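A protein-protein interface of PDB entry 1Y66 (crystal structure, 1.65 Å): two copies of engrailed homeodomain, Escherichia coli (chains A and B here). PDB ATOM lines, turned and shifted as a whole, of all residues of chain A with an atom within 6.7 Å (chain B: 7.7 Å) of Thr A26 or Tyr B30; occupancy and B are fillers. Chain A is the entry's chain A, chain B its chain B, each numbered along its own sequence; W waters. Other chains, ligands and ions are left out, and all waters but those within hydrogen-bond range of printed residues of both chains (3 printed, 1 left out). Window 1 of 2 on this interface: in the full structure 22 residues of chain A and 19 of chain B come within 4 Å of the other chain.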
ATOM      1  N   HIS A  19     -20.069 -10.549 -13.567  1.00  0.00           N
ATOM      2  CA  HIS A  19     -20.580 -11.860 -13.990  1.00  0.00           C
ATOM      3  C   HIS A  19     -19.556 -12.441 -14.989  1.00  0.00           C
ATOM      4  O   HIS A  19     -19.105 -13.618 -14.851  1.00  0.00           O
ATOM      5  CB  HIS A  19     -21.943 -11.694 -14.650  1.00  0.00           C
ATOM      6  CG  HIS A  19     -22.675 -12.996 -14.758  1.00  0.00           C
ATOM      7  ND1 HIS A  19     -23.771 -13.317 -13.980  1.00  0.00           N
ATOM      8  CD2 HIS A  19     -22.475 -14.046 -15.590  1.00  0.00           C
ATOM      9  CE1 HIS A  19     -24.185 -14.535 -14.290  1.00  0.00           C
ATOM     10  NE2 HIS A  19     -23.415 -14.999 -15.267  1.00  0.00           N
ATOM     11  N   GLU A  21     -16.364 -11.502 -15.299  1.00  0.00           N
ATOM     12  CA  GLU A  21     -15.075 -11.686 -14.617  1.00  0.00           C
ATOM     13  C   GLU A  21     -15.054 -13.038 -13.887  1.00  0.00           C
ATOM     14  O   GLU A  21     -14.045 -13.761 -13.951  1.00  0.00           O
ATOM     15  CB  GLU A  21     -14.817 -10.538 -13.638  1.00  0.00           C
ATOM     16  CG  GLU A  21     -13.541 -10.596 -12.905  1.00  0.00           C
ATOM     17  CD  GLU A  21     -13.456  -9.525 -11.842  1.00  0.00           C
ATOM     18  OE1 GLU A  21     -14.227  -8.542 -11.912  1.00  0.00           O
ATOM     19  OE2 GLU A  21     -12.626  -9.699 -10.908  1.00  0.00           O
ATOM     20  N   ILE A  22     -16.148 -13.349 -13.190  1.00  0.00           N
ATOM     21  CA  ILE A  22     -16.276 -14.598 -12.425  1.00  0.00           C
ATOM     22  C   ILE A  22     -16.239 -15.784 -13.401  1.00  0.00           C
ATOM     23  O   ILE A  22     -15.566 -16.809 -13.180  1.00  0.00           O
ATOM     24  CB  ILE A  22     -17.575 -14.605 -11.606  1.00  0.00           C
ATOM     25  CG1 ILE A  22     -17.474 -13.576 -10.455  1.00  0.00           C
ATOM     26  CG2 ILE A  22     -17.890 -16.019 -11.062  1.00  0.00           C
ATOM     27  CD1 ILE A  22     -18.841 -13.155  -9.874  1.00  0.00           C
ATOM     28  N   THR A  23     -16.926 -15.645 -14.514  1.00  0.00           N
ATOM     29  CA  THR A  23     -16.933 -16.741 -15.481  1.00  0.00           C
ATOM     30  C   THR A  23     -15.515 -16.962 -16.026  1.00  0.00           C
ATOM     31  O   THR A  23     -15.055 -18.097 -16.084  1.00  0.00           O
ATOM     32  CB  THR A  23     -17.885 -16.367 -16.614  1.00  0.00           C
ATOM     33  OG1 THR A  23     -19.223 -16.360 -16.093  1.00  0.00           O
ATOM     34  CG2 THR A  23     -17.808 -17.430 -17.736  1.00  0.00           C
ATOM     35  N   GLN A  24     -14.805 -15.895 -16.407  1.00  0.00           N
ATOM     36  CA  GLN A  24     -13.463 -16.063 -16.984  1.00  0.00           C
ATOM     37  C   GLN A  24     -12.507 -16.673 -15.953  1.00  0.00           C
ATOM     38  O   GLN A  24     -11.736 -17.594 -16.257  1.00  0.00           O
ATOM     39  CB  GLN A  24     -12.935 -14.708 -17.508  1.00  0.00           C
ATOM     40  CG  GLN A  24     -13.783 -14.149 -18.615  1.00  0.00           C
ATOM     41  CD  GLN A  24     -13.286 -12.776 -19.059  1.00  0.00           C
ATOM     42  OE1 GLN A  24     -13.337 -11.804 -18.300  1.00  0.00           O
ATOM     43  NE2 GLN A  24     -12.794 -12.695 -20.296  1.00  0.00           N
ATOM     44  N   GLU A  25     -12.600 -16.227 -14.708  1.00  0.00           N
ATOM     45  CA  GLU A  25     -11.687 -16.749 -13.697  1.00  0.00           C
ATOM     46  C   GLU A  25     -11.954 -18.255 -13.421  1.00  0.00           C
ATOM     47  O   GLU A  25     -11.028 -19.073 -13.266  1.00  0.00           O
ATOM     48  CB  GLU A  25     -11.783 -15.850 -12.476  1.00  0.00           C
ATOM     49  CG  GLU A  25     -12.883 -16.094 -11.572  1.00  0.00           C
ATOM     50  CD  GLU A  25     -12.798 -15.138 -10.361  1.00  0.00           C
ATOM     51  OE1 GLU A  25     -12.060 -14.121 -10.454  1.00  0.00           O
ATOM     52  OE2 GLU A  25     -13.465 -15.388  -9.354  1.00  0.00           O
ATOM     53  N   THR A  26     -13.230 -18.601 -13.429  1.00  0.00           N
ATOM     54  CA  THR A  26     -13.682 -19.983 -13.225  1.00  0.00           C
ATOM     55  C   THR A  26     -13.168 -20.865 -14.357  1.00  0.00           C
ATOM     56  O   THR A  26     -12.676 -21.967 -14.106  1.00  0.00           O
ATOM     57  CB  THR A  26     -15.218 -20.020 -13.110  1.00  0.00           C
ATOM     58  OG1 THR A  26     -15.561 -19.311 -11.920  1.00  0.00           O
ATOM     59  CG2 THR A  26     -15.729 -21.436 -12.963  1.00  0.00           C
ATOM     60  N   LEU A  27     -13.367 -20.430 -15.598  1.00  0.00           N
ATOM     61  CA  LEU A  27     -13.028 -21.281 -16.754  1.00  0.00           C
ATOM     62  C   LEU A  27     -11.516 -21.493 -16.787  1.00  0.00           C
ATOM     63  O   LEU A  27     -11.065 -22.597 -17.055  1.00  0.00           O
ATOM     64  CB  LEU A  27     -13.514 -20.603 -18.031  1.00  0.00           C
ATOM     65  CG  LEU A  27     -15.031 -20.628 -18.166  1.00  0.00           C
ATOM     66  CD1 LEU A  27     -15.372 -19.977 -19.451  1.00  0.00           C
ATOM     67  CD2 LEU A  27     -15.674 -22.073 -17.984  1.00  0.00           C
ATOM     68  N   HIS A  28     -10.730 -20.434 -16.499  1.00  0.00           N
ATOM     69  CA  HIS A  28      -9.296 -20.642 -16.372  1.00  0.00           C
ATOM     70  C   HIS A  28      -8.921 -21.601 -15.281  1.00  0.00           C
ATOM     71  O   HIS A  28      -8.051 -22.480 -15.515  1.00  0.00           O
ATOM     72  CB  HIS A  28      -8.574 -19.320 -16.227  1.00  0.00           C
ATOM     73  CG  HIS A  28      -8.348 -18.670 -17.539  1.00  0.00           C
ATOM     74  ND1 HIS A  28      -9.126 -17.640 -18.015  1.00  0.00           N
ATOM     75  CD2 HIS A  28      -7.486 -18.979 -18.531  1.00  0.00           C
ATOM     76  CE1 HIS A  28      -8.705 -17.289 -19.217  1.00  0.00           C
ATOM     77  NE2 HIS A  28      -7.743 -18.123 -19.572  1.00  0.00           N
ATOM     78  N   GLU A  29      -9.520 -21.468 -14.099  1.00  0.00           N
ATOM     79  CA  GLU A  29      -9.156 -22.354 -12.986  1.00  0.00           C
ATOM     80  C   GLU A  29      -9.497 -23.796 -13.341  1.00  0.00           C
ATOM     81  O   GLU A  29      -8.704 -24.733 -13.105  1.00  0.00           O
ATOM     82  CB  GLU A  29      -9.884 -21.965 -11.701  1.00  0.00           C
ATOM     83  CG  GLU A  29      -9.624 -22.935 -10.594  1.00  0.00           C
ATOM     84  CD  GLU A  29     -10.177 -22.465  -9.276  1.00  0.00           C
ATOM     85  OE1 GLU A  29     -10.174 -21.247  -9.006  1.00  0.00           O
ATOM     86  OE2 GLU A  29     -10.628 -23.317  -8.481  1.00  0.00           O
ATOM     87  N   TYR A  30     -10.649 -23.968 -13.959  1.00  0.00           N
ATOM     88  CA  TYR A  30     -11.086 -25.291 -14.377  1.00  0.00           C
ATOM     89  C   TYR A  30     -10.099 -25.889 -15.370  1.00  0.00           C
ATOM     90  O   TYR A  30      -9.684 -27.040 -15.205  1.00  0.00           O
ATOM     91  CB  TYR A  30     -12.452 -25.186 -15.029  1.00  0.00           C
ATOM     92  CG  TYR A  30     -13.065 -26.507 -15.382  1.00  0.00           C
ATOM     93  CD1 TYR A  30     -13.160 -27.599 -14.451  1.00  0.00           C
ATOM     94  CD2 TYR A  30     -13.608 -26.694 -16.671  1.00  0.00           C
ATOM     95  CE1 TYR A  30     -13.778 -28.809 -14.800  1.00  0.00           C
ATOM     96  CE2 TYR A  30     -14.233 -27.864 -17.051  1.00  0.00           C
ATOM     97  CZ  TYR A  30     -14.333 -28.985 -16.131  1.00  0.00           C
ATOM     98  OH  TYR A  30     -14.963 -30.168 -16.548  1.00  0.00           O
ATOM     99  N   ALA A  31      -9.712 -25.135 -16.384  1.00  0.00           N
ATOM    100  CA  ALA A  31      -8.768 -25.643 -17.356  1.00  0.00           C
ATOM    101  C   ALA A  31      -7.420 -26.000 -16.723  1.00  0.00           C
ATOM    102  O   ALA A  31      -6.804 -26.987 -17.112  1.00  0.00           O
ATOM    103  CB  ALA A  31      -8.589 -24.625 -18.493  1.00  0.00           C
ATOM    104  N   THR B  23     -14.951 -31.242 -11.864  1.00  0.00           N
ATOM    105  CA  THR B  23     -16.060 -30.566 -12.508  1.00  0.00           C
ATOM    106  C   THR B  23     -17.128 -30.168 -11.504  1.00  0.00           C
ATOM    107  O   THR B  23     -17.642 -29.035 -11.538  1.00  0.00           O
ATOM    108  CB  THR B  23     -16.693 -31.503 -13.554  1.00  0.00           C
ATOM    109  OG1 THR B  23     -15.671 -31.860 -14.480  1.00  0.00           O
ATOM    110  CG2 THR B  23     -17.792 -30.750 -14.356  1.00  0.00           C
ATOM    111  N   GLN B  24     -17.498 -31.098 -10.616  1.00  0.00           N
ATOM    112  CA  GLN B  24     -18.542 -30.854  -9.623  1.00  0.00           C
ATOM    113  C   GLN B  24     -18.121 -29.749  -8.649  1.00  0.00           C
ATOM    114  O   GLN B  24     -18.884 -28.819  -8.375  1.00  0.00           O
ATOM    115  CB  GLN B  24     -18.868 -32.156  -8.889  1.00  0.00           C
ATOM    116  CG  GLN B  24     -19.955 -32.009  -7.923  1.00  0.00           C
ATOM    117  CD  GLN B  24     -21.337 -32.136  -8.555  1.00  0.00           C
ATOM    118  OE1 GLN B  24     -21.556 -31.822  -9.750  1.00  0.00           O
ATOM    119  NE2 GLN B  24     -22.281 -32.595  -7.763  1.00  0.00           N
ATOM    120  N   GLU B  25     -16.872 -29.801  -8.191  1.00  0.00           N
ATOM    121  CA  GLU B  25     -16.423 -28.772  -7.246  1.00  0.00           C
ATOM    122  C   GLU B  25     -16.333 -27.405  -7.938  1.00  0.00           C
ATOM    123  O   GLU B  25     -16.621 -26.369  -7.324  1.00  0.00           O
ATOM    124  CB  GLU B  25     -15.066 -29.150  -6.664  1.00  0.00           C
ATOM    125  CG  GLU B  25     -15.081 -30.337  -5.686  1.00  0.00           C
ATOM    126  CD  GLU B  25     -16.112 -30.211  -4.555  1.00  0.00           C
ATOM    127  OE1 GLU B  25     -16.536 -29.097  -4.159  1.00  0.00           O
ATOM    128  OE2 GLU B  25     -16.472 -31.264  -4.007  1.00  0.00           O
ATOM    129  N   THR B  26     -15.954 -27.417  -9.212  1.00  0.00           N
ATOM    130  CA  THR B  26     -15.800 -26.162  -9.957  1.00  0.00           C
ATOM    131  C   THR B  26     -17.201 -25.539 -10.122  1.00  0.00           C
ATOM    132  O   THR B  26     -17.394 -24.337  -9.945  1.00  0.00           O
ATOM    133  CB  THR B  26     -15.128 -26.431 -11.296  1.00  0.00           C
ATOM    134  OG1 THR B  26     -13.735 -26.736 -11.043  1.00  0.00           O
ATOM    135  CG2 THR B  26     -15.181 -25.157 -12.214  1.00  0.00           C
ATOM    136  N   LEU B  27     -18.170 -26.376 -10.473  1.00  0.00           N
ATOM    137  CA  LEU B  27     -19.557 -25.901 -10.585  1.00  0.00           C
ATOM    138  C   LEU B  27     -20.065 -25.336  -9.271  1.00  0.00           C
ATOM    139  O   LEU B  27     -20.703 -24.291  -9.259  1.00  0.00           O
ATOM    140  CB  LEU B  27     -20.465 -27.070 -11.036  1.00  0.00           C
ATOM    141  CG  LEU B  27     -20.426 -27.337 -12.515  1.00  0.00           C
ATOM    142  CD1 LEU B  27     -21.116 -28.671 -12.794  1.00  0.00           C
ATOM    143  CD2 LEU B  27     -21.140 -26.208 -13.322  1.00  0.00           C
ATOM    144  N   HIS B  28     -19.741 -25.990  -8.152  1.00  0.00           N
ATOM    145  CA  HIS B  28     -20.219 -25.473  -6.849  1.00  0.00           C
ATOM    146  C   HIS B  28     -19.599 -24.112  -6.559  1.00  0.00           C
ATOM    147  O   HIS B  28     -20.291 -23.189  -6.078  1.00  0.00           O
ATOM    148  CB  HIS B  28     -19.874 -26.422  -5.727  1.00  0.00           C
ATOM    149  CG  HIS B  28     -20.607 -27.730  -5.813  1.00  0.00           C
ATOM    150  ND1 HIS B  28     -20.121 -28.898  -5.246  1.00  0.00           N
ATOM    151  CD2 HIS B  28     -21.752 -28.062  -6.435  1.00  0.00           C
ATOM    152  CE1 HIS B  28     -20.971 -29.880  -5.481  1.00  0.00           C
ATOM    153  NE2 HIS B  28     -21.962 -29.410  -6.215  1.00  0.00           N
ATOM    154  N   GLU B  29     -18.295 -23.999  -6.801  1.00  0.00           N
ATOM    155  CA  GLU B  29     -17.575 -22.772  -6.514  1.00  0.00           C
ATOM    156  C   GLU B  29     -18.097 -21.647  -7.406  1.00  0.00           C
ATOM    157  O   GLU B  29     -18.306 -20.530  -6.946  1.00  0.00           O
ATOM    158  CB  GLU B  29     -16.091 -23.010  -6.744  1.00  0.00           C
ATOM    159  CG  GLU B  29     -15.251 -21.720  -6.490  1.00  0.00           C
ATOM    160  CD  GLU B  29     -13.760 -21.980  -6.570  1.00  0.00           C
ATOM    161  OE1 GLU B  29     -13.348 -23.142  -6.760  1.00  0.00           O
ATOM    162  OE2 GLU B  29     -12.992 -21.002  -6.519  1.00  0.00           O
ATOM    163  N   TYR B  30     -18.323 -21.971  -8.670  1.00  0.00           N
ATOM    164  CA  TYR B  30     -18.846 -20.989  -9.647  1.00  0.00           C
ATOM    165  C   TYR B  30     -20.208 -20.475  -9.201  1.00  0.00           C
ATOM    166  O   TYR B  30     -20.456 -19.280  -9.185  1.00  0.00           O
ATOM    167  CB  TYR B  30     -18.927 -21.679 -11.000  1.00  0.00           C
ATOM    168  CG  TYR B  30     -19.289 -20.825 -12.178  1.00  0.00           C
ATOM    169  CD1 TYR B  30     -18.911 -19.478 -12.287  1.00  0.00           C
ATOM    170  CD2 TYR B  30     -19.946 -21.421 -13.267  1.00  0.00           C
ATOM    171  CE1 TYR B  30     -19.250 -18.743 -13.470  1.00  0.00           C
ATOM    172  CE2 TYR B  30     -20.254 -20.733 -14.428  1.00  0.00           C
ATOM    173  CZ  TYR B  30     -19.909 -19.390 -14.540  1.00  0.00           C
ATOM    174  OH  TYR B  30     -20.213 -18.713 -15.716  1.00  0.00           O
ATOM    175  N   ALA B  31     -21.093 -21.392  -8.824  1.00  0.00           N
ATOM    176  CA  ALA B  31     -22.431 -21.037  -8.337  1.00  0.00           C
ATOM    177  C   ALA B  31     -22.333 -20.123  -7.111  1.00  0.00           C
ATOM    178  O   ALA B  31     -23.104 -19.161  -6.986  1.00  0.00           O
ATOM    179  CB  ALA B  31     -23.171 -22.334  -7.971  1.00  0.00           C
ATOM    180  N   GLN B  32     -21.408 -20.424  -6.191  1.00  0.00           N
ATOM    181  CA  GLN B  32     -21.264 -19.653  -4.976  1.00  0.00           C
ATOM    182  C   GLN B  32     -20.851 -18.231  -5.343  1.00  0.00           C
ATOM    183  O   GLN B  32     -21.426 -17.273  -4.834  1.00  0.00           O
ATOM    184  CB  GLN B  32     -20.240 -20.288  -4.038  1.00  0.00           C
ATOM    185  CG  GLN B  32     -20.207 -19.604  -2.704  1.00  0.00           C
ATOM    186  N   LYS B  33     -19.900 -18.097  -6.264  1.00  0.00           N
ATOM    187  CA  LYS B  33     -19.379 -16.773  -6.614  1.00  0.00           C
ATOM    188  C   LYS B  33     -20.415 -15.972  -7.370  1.00  0.00           C
ATOM    189  O   LYS B  33     -20.602 -14.771  -7.083  1.00  0.00           O
ATOM    190  CB  LYS B  33     -18.097 -16.918  -7.471  1.00  0.00           C
ATOM    191  CG  LYS B  33     -16.939 -17.347  -6.593  1.00  0.00           C
ATOM    192  CD  LYS B  33     -15.682 -17.443  -7.330  1.00  0.00           C
ATOM    193  CE  LYS B  33     -14.612 -17.979  -6.370  1.00  0.00           C
ATOM    194  NZ  LYS B  33     -13.337 -18.178  -7.087  1.00  0.00           N
ATOM    195  N   LEU B  34     -21.105 -16.607  -8.321  1.00  0.00           N
ATOM    196  CA  LEU B  34     -22.192 -15.870  -8.988  1.00  0.00           C
ATOM    197  C   LEU B  34     -23.284 -15.498  -8.010  1.00  0.00           C
ATOM    198  O   LEU B  34     -23.923 -14.426  -8.153  1.00  0.00           O
ATOM    199  CB  LEU B  34     -22.779 -16.647 -10.173  1.00  0.00           C
ATOM    200  CG  LEU B  34     -21.810 -16.911 -11.322  1.00  0.00           C
ATOM    201  CD1 LEU B  34     -22.537 -17.735 -12.401  1.00  0.00           C
ATOM    202  CD2 LEU B  34     -21.282 -15.619 -11.934  1.00  0.00           C
ATOM    203  N   GLY B  35     -23.528 -16.375  -7.030  1.00  0.00           N
ATOM    204  CA  GLY B  35     -24.545 -16.098  -6.016  1.00  0.00           C
ATOM    205  C   GLY B  35     -24.200 -14.827  -5.270  1.00  0.00           C
ATOM    206  O   GLY B  35     -25.073 -13.987  -5.033  1.00  0.00           O
ATOM    207  N   LEU B  36     -22.943 -14.686  -4.871  1.00  0.00           N
ATOM    208  CA  LEU B  36     -22.553 -13.509  -4.107  1.00  0.00           C
ATOM    209  C   LEU B  36     -22.784 -12.236  -4.972  1.00  0.00           C
ATOM    210  O   LEU B  36     -23.263 -11.181  -4.463  1.00  0.00           O
ATOM    211  CB  LEU B  36     -21.106 -13.644  -3.674  1.00  0.00           C
ATOM    212  CG  LEU B  36     -20.880 -14.618  -2.522  1.00  0.00           C
ATOM    213  CD1 LEU B  36     -19.410 -14.630  -2.270  1.00  0.00           C
ATOM    214  CD2 LEU B  36     -21.650 -14.182  -1.254  1.00  0.00           C
HETATM  215  O   HOH W   1     -14.478 -20.301  -9.589  1.00  0.00           O
HETATM  216  O   HOH W   2     -11.757 -19.140  -9.499  1.00  0.00           O
HETATM  217  O   HOH W   3     -24.143 -13.160 -10.611  1.00  0.00           O
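OH of Tyr B30 lies within hydrogen-bond range of OG1 of Thr A23.
OE2 of Glu A25 lies within salt-bridge range of NZ of Lys B33 (3.6 Å).
The side-chain hydroxyl (OH) of Tyr A30 is in hydrogen-bond range of the side-chain hydroxyl (OG1) of Thr B23, 2.8 Å away.
The side-chain carboxylate (OE2) of Glu A29 lies close to the side-chain carboxylate (OE1) of Glu B29, 3.2 Å away.
The side-chain hydroxyl (OG1) of Thr A23 is in hydrogen-bond range of the backbone carbonyl oxygen (O) of His A19.
The backbone carbonyl oxygen (O) of Ile A22 is in hydrogen-bond range of the side-chain hydroxyl (OG1) of Thr A26.
OE2 of Glu B29 sits close to NZ of Lys B33, at 2.9 Å.
Among the printed residues, merely in contact across the chains: His A19 with Leu B34, Ile A22 with Tyr B30, Ile A22 with Lys B33, Ile A22 with Leu B34, Thr A26 with Thr B26, Thr A26 with Tyr B30 and Tyr A30 with Thr B26.
Thr A26 touches just these residues of chain B: Thr B26 (3.8 Å) and Tyr B30 (3.4 Å).
Of the printed residues of chain A, Leu B34 touches His A19 (3.9 Å) and Ile A22 (3.5 Å).
Printed residues of chain A within 4 Å of Lys B33: Ile A22 and Glu A25.
Of the printed residues of chain A, Glu B29 touches Glu A29.
Printed residues of chain B within 4 Å of Glu A29: Glu B29 (3.2 Å).
The nearest residue of chain B that does not touch Thr A26 is Lys B33 (5.0 Å).
The nearest residue of chain A that does not touch Tyr B30 is His A19 (4.9 Å).
The nearest printed residue of chain A that does not touch Lys B33 is Glu A29 (4.8 Å).
Of the 14 printed residues of chain B, 6 touch a printed residue of chain A.
Hydrophobic or aromatic side chains of chain B within 4 Å of the printed part of chain A: Tyr B30 and Leu B34.
Of the 12 printed residues of chain A, 7 touch a printed residue of chain B.
Hydrophobic or aromatic side chains of chain A that line the printed part of chain B: His A19, Ile A22 and Tyr A30.
Along chain A the printed residues that touch a printed residue of chain B span positions 19 to 30.
Thr A23 touches Tyr B30, and with the chains exchanged Tyr A30 touches Thr B23.
Thr B26 touches its own counterpart, Thr A26.
Thr A26 touches Tyr B30, and with the chains exchanged Tyr A30 touches Thr B26.
Glu B29 touches its own counterpart, Glu A29.
Of the 11 pairs that touch across the chains among the printed residues, 6 have their exchanged pair printed and touching as well.
Water W2 lies within hydrogen-bond range of OE1 of Glu A29 (2.7 Å) and NZ of Lys B33 (3.0 Å).
Water W1 lies within hydrogen-bond range of OG1 of Thr A26 and NZ of Lys B33.
Water W3 bridges the backbone carbonyl oxygen of Leu B34 and a ring nitrogen (ND1) of His A19.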
